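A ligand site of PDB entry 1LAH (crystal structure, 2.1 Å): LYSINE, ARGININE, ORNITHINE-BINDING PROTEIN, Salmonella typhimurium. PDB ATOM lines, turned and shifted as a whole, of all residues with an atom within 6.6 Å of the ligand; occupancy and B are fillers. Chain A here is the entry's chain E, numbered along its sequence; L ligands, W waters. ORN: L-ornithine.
A nitrogen (NE) of the ligand lies within hydrogen-bond range of the backbone carbonyl oxygen (O) of Ser 69, 2.8 Å away.
An oxygen (O) of the ligand lies within salt-bridge range of the guanidinium group (NH1) of Arg 77 (2.8 Å).
N of Ser 72 is in hydrogen-bond range of O of the ligand (2.9 Å).
A nitrogen (N) of the ligand is in hydrogen-bond range of the side-chain hydroxyl (OG) of Ser 72 (3.0 Å).
N of the ligand is in hydrogen-bond range of O of Ser 70, 2.9 Å away.
The backbone NH (N) of Thr 121 is in hydrogen-bond range of an oxygen (OXT) of the ligand (3.0 Å).
A nitrogen (NE) of the ligand is in salt-bridge range of the side-chain carboxylate of Asp 11, 3.0 Å away.
OD2 of Asp 161 is in salt-bridge range of N of the ligand, 3.0 Å away.
The side-chain hydroxyl (OG) of Ser 69 is in hydrogen-bond range of the backbone NH (N) of Asp 11, 3.1 Å away.
O of Ser 72 is in hydrogen-bond range of NH1 of Arg 77, 3.0 Å away.
The backbone carbonyl oxygen (O) of Gly 119 is in hydrogen-bond range of the guanidinium group (NH2) of Arg 77 (3.4 Å).
The side-chain hydroxyl (OG1) of Thr 121 lies within hydrogen-bond range of the side-chain amide oxygen (OE1) of Gln 122 (3.5 Å).
The side-chain carboxylate of Asp 161 lies within hydrogen-bond range of the side-chain amide nitrogen of Gln 122, 2.9 Å away.
OH of Tyr 14 lies within hydrogen-bond range of N of Asp 161, 3.1 Å away.
The side-chain hydroxyl (OG) of Ser 120 lies close to the side-chain amide oxygen (OE1) of Gln 122 (3.3 Å).
The side-chain amide nitrogen (NE2) of Gln 122 lies within hydrogen-bond range of the side-chain hydroxyl (OG) of Ser 92 (2.7 Å).
Residues that only touch the ligand: Tyr 14 (3.6 Å), Phe 52 (3.4 Å), Leu 71 (3.7 Å), Leu 117 (3.7 Å), Ser 120 (3.2 Å) and Gln 122 (3.5 Å).
Of the 23 residues printed, 13 come within 4 Å of the ligand.
The nearest printed residue that does not touch the ligand is Gly 119 (4.5 Å).
Water W1 lies within hydrogen-bond range of OD1 of Asp 11 (2.7 Å), OG of Ser 69 (2.7 Å) and NE of the ligand (2.7 Å).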
ATOM      1  N   ASP A  11      -4.412  19.177   8.378  1.00  0.00           N
ATOM      2  CA  ASP A  11      -5.105  18.935   7.128  1.00  0.00           C
ATOM      3  C   ASP A  11      -6.393  18.120   7.253  1.00  0.00           C
ATOM      4  O   ASP A  11      -7.204  18.139   6.333  1.00  0.00           O
ATOM      5  CB  ASP A  11      -4.151  18.270   6.098  1.00  0.00           C
ATOM      6  CG  ASP A  11      -3.619  16.859   6.401  1.00  0.00           C
ATOM      7  OD1 ASP A  11      -4.140  16.205   7.292  1.00  0.00           O
ATOM      8  OD2 ASP A  11      -2.691  16.396   5.757  1.00  0.00           O
ATOM      9  N   THR A  13      -7.051  15.091   6.934  1.00  0.00           N
ATOM     10  CA  THR A  13      -7.172  13.917   6.094  1.00  0.00           C
ATOM     11  C   THR A  13      -5.961  12.972   6.245  1.00  0.00           C
ATOM     12  O   THR A  13      -5.383  12.507   5.263  1.00  0.00           O
ATOM     13  CB  THR A  13      -7.359  14.465   4.665  1.00  0.00           C
ATOM     14  OG1 THR A  13      -6.441  15.538   4.407  1.00  0.00           O
ATOM     15  CG2 THR A  13      -8.793  14.973   4.522  1.00  0.00           C
ATOM     16  N   TYR A  14      -5.528  12.658   7.446  1.00  0.00           N
ATOM     17  CA  TYR A  14      -4.330  11.864   7.601  1.00  0.00           C
ATOM     18  C   TYR A  14      -4.459  11.056   8.892  1.00  0.00           C
ATOM     19  O   TYR A  14      -3.709  11.215   9.864  1.00  0.00           O
ATOM     20  CB  TYR A  14      -3.101  12.832   7.608  1.00  0.00           C
ATOM     21  CG  TYR A  14      -1.863  12.315   6.890  1.00  0.00           C
ATOM     22  CD1 TYR A  14      -1.889  12.243   5.505  1.00  0.00           C
ATOM     23  CD2 TYR A  14      -0.740  11.932   7.608  1.00  0.00           C
ATOM     24  CE1 TYR A  14      -0.784  11.782   4.808  1.00  0.00           C
ATOM     25  CE2 TYR A  14       0.365  11.470   6.911  1.00  0.00           C
ATOM     26  CZ  TYR A  14       0.329  11.397   5.527  1.00  0.00           C
ATOM     27  OH  TYR A  14       1.427  10.916   4.843  1.00  0.00           O
ATOM     28  N   PHE A  52      -3.143  20.418   2.953  1.00  0.00           N
ATOM     29  CA  PHE A  52      -1.802  20.319   3.492  1.00  0.00           C
ATOM     30  C   PHE A  52      -0.870  21.293   2.834  1.00  0.00           C
ATOM     31  O   PHE A  52      -0.098  21.917   3.548  1.00  0.00           O
ATOM     32  CB  PHE A  52      -1.256  18.911   3.291  1.00  0.00           C
ATOM     33  CG  PHE A  52       0.128  18.741   3.886  1.00  0.00           C
ATOM     34  CD1 PHE A  52       0.267  18.665   5.265  1.00  0.00           C
ATOM     35  CD2 PHE A  52       1.225  18.651   3.057  1.00  0.00           C
ATOM     36  CE1 PHE A  52       1.525  18.503   5.826  1.00  0.00           C
ATOM     37  CE2 PHE A  52       2.474  18.488   3.619  1.00  0.00           C
ATOM     38  CZ  PHE A  52       2.623  18.412   4.997  1.00  0.00           C
ATOM     39  N   LEU A  55      -0.703  24.927   4.306  1.00  0.00           N
ATOM     40  CA  LEU A  55      -0.394  25.136   5.708  1.00  0.00           C
ATOM     41  C   LEU A  55       0.834  26.022   5.915  1.00  0.00           C
ATOM     42  O   LEU A  55       0.760  27.049   6.609  1.00  0.00           O
ATOM     43  CB  LEU A  55      -0.216  23.754   6.400  1.00  0.00           C
ATOM     44  CG  LEU A  55      -1.472  22.854   6.657  1.00  0.00           C
ATOM     45  CD1 LEU A  55      -1.095  21.494   7.246  1.00  0.00           C
ATOM     46  CD2 LEU A  55      -2.381  23.540   7.656  1.00  0.00           C
ATOM     47  N   SER A  69       0.460  18.657  11.824  1.00  0.00           N
ATOM     48  CA  SER A  69      -0.139  17.928  10.762  1.00  0.00           C
ATOM     49  C   SER A  69       0.857  16.907  10.193  1.00  0.00           C
ATOM     50  O   SER A  69       0.991  16.795   8.947  1.00  0.00           O
ATOM     51  CB  SER A  69      -0.565  18.949   9.736  1.00  0.00           C
ATOM     52  OG  SER A  69      -1.506  18.322   8.856  1.00  0.00           O
ATOM     53  N   SER A  70       1.548  16.150  11.091  1.00  0.00           N
ATOM     54  CA  SER A  70       2.607  15.171  10.755  1.00  0.00           C
ATOM     55  C   SER A  70       3.637  15.844   9.827  1.00  0.00           C
ATOM     56  O   SER A  70       4.066  15.296   8.804  1.00  0.00           O
ATOM     57  CB  SER A  70       2.038  13.941  10.026  1.00  0.00           C
ATOM     58  OG  SER A  70       1.086  13.116  10.712  1.00  0.00           O
ATOM     59  N   LEU A  71       4.002  17.065  10.176  1.00  0.00           N
ATOM     60  CA  LEU A  71       4.922  17.883   9.371  1.00  0.00           C
ATOM     61  C   LEU A  71       6.383  17.429   9.615  1.00  0.00           C
ATOM     62  O   LEU A  71       6.935  17.587  10.715  1.00  0.00           O
ATOM     63  CB  LEU A  71       4.718  19.355   9.796  1.00  0.00           C
ATOM     64  CG  LEU A  71       5.385  20.366   8.870  1.00  0.00           C
ATOM     65  CD1 LEU A  71       4.696  20.416   7.518  1.00  0.00           C
ATOM     66  CD2 LEU A  71       5.287  21.722   9.515  1.00  0.00           C
ATOM     67  N   SER A  72       7.001  16.809   8.599  1.00  0.00           N
ATOM     68  CA  SER A  72       8.344  16.279   8.718  1.00  0.00           C
ATOM     69  C   SER A  72       9.338  17.410   8.833  1.00  0.00           C
ATOM     70  O   SER A  72       9.212  18.401   8.122  1.00  0.00           O
ATOM     71  CB  SER A  72       8.638  15.413   7.503  1.00  0.00           C
ATOM     72  OG  SER A  72       7.931  14.162   7.599  1.00  0.00           O
ATOM     73  N   ILE A  73      10.245  17.300   9.823  1.00  0.00           N
ATOM     74  CA  ILE A  73      11.326  18.260  10.041  1.00  0.00           C
ATOM     75  C   ILE A  73      12.407  17.959   8.984  1.00  0.00           C
ATOM     76  O   ILE A  73      13.090  16.929   9.049  1.00  0.00           O
ATOM     77  CB  ILE A  73      11.941  18.115  11.464  1.00  0.00           C
ATOM     78  CG1 ILE A  73      10.841  18.166  12.521  1.00  0.00           C
ATOM     79  CG2 ILE A  73      12.992  19.236  11.635  1.00  0.00           C
ATOM     80  CD1 ILE A  73      11.238  17.715  13.916  1.00  0.00           C
ATOM     81  N   THR A  74      12.512  18.783   7.947  1.00  0.00           N
ATOM     82  CA  THR A  74      13.432  18.554   6.866  1.00  0.00           C
ATOM     83  C   THR A  74      14.321  19.780   6.832  1.00  0.00           C
ATOM     84  O   THR A  74      13.955  20.867   7.314  1.00  0.00           O
ATOM     85  CB  THR A  74      12.708  18.425   5.514  1.00  0.00           C
ATOM     86  OG1 THR A  74      12.077  19.672   5.279  1.00  0.00           O
ATOM     87  CG2 THR A  74      11.716  17.261   5.486  1.00  0.00           C
ATOM     88  N   ARG A  77      12.477  22.567   4.800  1.00  0.00           N
ATOM     89  CA  ARG A  77      11.485  23.370   5.505  1.00  0.00           C
ATOM     90  C   ARG A  77      12.129  24.254   6.551  1.00  0.00           C
ATOM     91  O   ARG A  77      11.645  25.366   6.805  1.00  0.00           O
ATOM     92  CB  ARG A  77      10.475  22.492   6.178  1.00  0.00           C
ATOM     93  CG  ARG A  77       9.534  21.980   5.120  1.00  0.00           C
ATOM     94  CD  ARG A  77       8.680  20.860   5.637  1.00  0.00           C
ATOM     95  NE  ARG A  77       7.808  20.363   4.576  1.00  0.00           N
ATOM     96  CZ  ARG A  77       7.137  19.213   4.719  1.00  0.00           C
ATOM     97  NH1 ARG A  77       7.224  18.460   5.818  1.00  0.00           N
ATOM     98  NH2 ARG A  77       6.371  18.776   3.752  1.00  0.00           N
ATOM     99  N   ALA A  90       8.503   9.364  11.409  1.00  0.00           N
ATOM    100  CA  ALA A  90       7.715   9.043  10.244  1.00  0.00           C
ATOM    101  C   ALA A  90       8.514   8.623   9.013  1.00  0.00           C
ATOM    102  O   ALA A  90       9.113   9.445   8.324  1.00  0.00           O
ATOM    103  CB  ALA A  90       6.897  10.237   9.827  1.00  0.00           C
ATOM    104  N   SER A  92       8.363   6.785   5.102  1.00  0.00           N
ATOM    105  CA  SER A  92       7.450   6.675   3.973  1.00  0.00           C
ATOM    106  C   SER A  92       7.467   5.250   3.453  1.00  0.00           C
ATOM    107  O   SER A  92       8.476   4.566   3.637  1.00  0.00           O
ATOM    108  CB  SER A  92       7.860   7.620   2.867  1.00  0.00           C
ATOM    109  OG  SER A  92       7.669   8.926   3.364  1.00  0.00           O
ATOM    110  N   LEU A 117       0.636  13.087  -1.933  1.00  0.00           N
ATOM    111  CA  LEU A 117      -0.036  14.278  -1.490  1.00  0.00           C
ATOM    112  C   LEU A 117       0.741  15.502  -1.986  1.00  0.00           C
ATOM    113  O   LEU A 117       1.932  15.637  -1.703  1.00  0.00           O
ATOM    114  CB  LEU A 117      -0.082  14.295   0.016  1.00  0.00           C
ATOM    115  CG  LEU A 117      -0.672  15.499   0.754  1.00  0.00           C
ATOM    116  CD1 LEU A 117      -2.153  15.672   0.466  1.00  0.00           C
ATOM    117  CD2 LEU A 117      -0.478  15.258   2.223  1.00  0.00           C
ATOM    118  N   GLY A 119       2.393  18.850  -1.916  1.00  0.00           N
ATOM    119  CA  GLY A 119       3.081  19.642  -0.912  1.00  0.00           C
ATOM    120  C   GLY A 119       3.834  18.792   0.096  1.00  0.00           C
ATOM    121  O   GLY A 119       4.415  19.340   1.034  1.00  0.00           O
ATOM    122  N   SER A 120       3.815  17.469  -0.029  1.00  0.00           N
ATOM    123  CA  SER A 120       4.434  16.648   0.985  1.00  0.00           C
ATOM    124  C   SER A 120       5.891  16.392   0.625  1.00  0.00           C
ATOM    125  O   SER A 120       6.359  16.665  -0.489  1.00  0.00           O
ATOM    126  CB  SER A 120       3.717  15.299   1.104  1.00  0.00           C
ATOM    127  OG  SER A 120       3.716  14.582  -0.111  1.00  0.00           O
ATOM    128  N   THR A 121       6.559  15.669   1.526  1.00  0.00           N
ATOM    129  CA  THR A 121       7.917  15.249   1.233  1.00  0.00           C
ATOM    130  C   THR A 121       7.899  14.146   0.194  1.00  0.00           C
ATOM    131  O   THR A 121       8.830  14.035  -0.609  1.00  0.00           O
ATOM    132  CB  THR A 121       8.608  14.764   2.522  1.00  0.00           C
ATOM    133  OG1 THR A 121       7.769  13.741   3.074  1.00  0.00           O
ATOM    134  CG2 THR A 121       8.913  15.923   3.465  1.00  0.00           C
ATOM    135  N   GLN A 122       6.803  13.354   0.157  1.00  0.00           N
ATOM    136  CA  GLN A 122       6.641  12.267  -0.800  1.00  0.00           C
ATOM    137  C   GLN A 122       6.485  12.846  -2.202  1.00  0.00           C
ATOM    138  O   GLN A 122       7.034  12.298  -3.149  1.00  0.00           O
ATOM    139  CB  GLN A 122       5.427  11.411  -0.498  1.00  0.00           C
ATOM    140  CG  GLN A 122       5.518  10.602   0.779  1.00  0.00           C
ATOM    141  CD  GLN A 122       5.269  11.361   2.051  1.00  0.00           C
ATOM    142  OE1 GLN A 122       4.699  12.453   2.151  1.00  0.00           O
ATOM    143  NE2 GLN A 122       5.696  10.744   3.132  1.00  0.00           N
ATOM    144  N   GLN A 160       3.212   7.558   0.978  1.00  0.00           N
ATOM    145  CA  GLN A 160       2.800   8.384   2.104  1.00  0.00           C
ATOM    146  C   GLN A 160       3.538   7.855   3.333  1.00  0.00           C
ATOM    147  O   GLN A 160       4.356   6.922   3.233  1.00  0.00           O
ATOM    148  CB  GLN A 160       1.268   8.309   2.348  1.00  0.00           C
ATOM    149  CG  GLN A 160       0.618   6.900   2.561  1.00  0.00           C
ATOM    150  CD  GLN A 160       0.582   6.052   1.292  1.00  0.00           C
ATOM    151  OE1 GLN A 160      -0.016   6.446   0.313  1.00  0.00           O
ATOM    152  NE2 GLN A 160       1.249   4.920   1.127  1.00  0.00           N
ATOM    153  N   ASP A 161       3.283   8.512   4.468  1.00  0.00           N
ATOM    154  CA  ASP A 161       3.864   8.073   5.720  1.00  0.00           C
ATOM    155  C   ASP A 161       3.313   6.696   6.034  1.00  0.00           C
ATOM    156  O   ASP A 161       2.086   6.469   5.986  1.00  0.00           O
ATOM    157  CB  ASP A 161       3.506   9.013   6.874  1.00  0.00           C
ATOM    158  CG  ASP A 161       4.188  10.371   6.815  1.00  0.00           C
ATOM    159  OD1 ASP A 161       5.021  10.590   5.941  1.00  0.00           O
ATOM    160  OD2 ASP A 161       3.880  11.247   7.644  1.00  0.00           O
ATOM    161  N   PHE A 191      13.000  13.065   3.446  1.00  0.00           N
ATOM    162  CA  PHE A 191      12.005  12.799   4.461  1.00  0.00           C
ATOM    163  C   PHE A 191      12.250  13.359   5.834  1.00  0.00           C
ATOM    164  O   PHE A 191      11.416  13.181   6.736  1.00  0.00           O
ATOM    165  CB  PHE A 191      11.811  11.285   4.518  1.00  0.00           C
ATOM    166  CG  PHE A 191      11.374  10.742   3.152  1.00  0.00           C
ATOM    167  CD1 PHE A 191      10.266  11.264   2.497  1.00  0.00           C
ATOM    168  CD2 PHE A 191      12.139   9.755   2.524  1.00  0.00           C
ATOM    169  CE1 PHE A 191       9.919  10.772   1.256  1.00  0.00           C
ATOM    170  CE2 PHE A 191      11.761   9.266   1.278  1.00  0.00           C
ATOM    171  CZ  PHE A 191      10.644   9.774   0.627  1.00  0.00           C
ATOM    172  N   THR A 195       8.550  14.332  12.858  1.00  0.00           N
ATOM    173  CA  THR A 195       7.645  15.440  12.591  1.00  0.00           C
ATOM    174  C   THR A 195       7.702  16.340  13.818  1.00  0.00           C
ATOM    175  O   THR A 195       8.114  15.905  14.910  1.00  0.00           O
ATOM    176  CB  THR A 195       6.163  14.864  12.339  1.00  0.00           C
ATOM    177  OG1 THR A 195       5.680  14.349  13.589  1.00  0.00           O
ATOM    178  CG2 THR A 195       6.125  13.696  11.344  1.00  0.00           C
HETATM  179  N   ORN L   1       5.148  13.770   6.602  1.00  0.00           N
HETATM  180  CA  ORN L   1       4.730  14.095   5.273  1.00  0.00           C
HETATM  181  CB  ORN L   1       3.193  14.012   5.104  1.00  0.00           C
HETATM  182  CG  ORN L   1       2.288  14.643   6.188  1.00  0.00           C
HETATM  183  CD  ORN L   1       0.953  15.057   5.585  1.00  0.00           C
HETATM  184  NE  ORN L   1       0.032  15.572   6.609  1.00  0.00           N
HETATM  185  C   ORN L   1       5.195  15.564   5.165  1.00  0.00           C
HETATM  186  O   ORN L   1       5.613  16.176   6.147  1.00  0.00           O
HETATM  187  OXT ORN L   1       5.128  16.096   4.078  1.00  0.00           O
HETATM  188  O   HOH W   1      -1.843  15.682   8.552  1.00  0.00           O
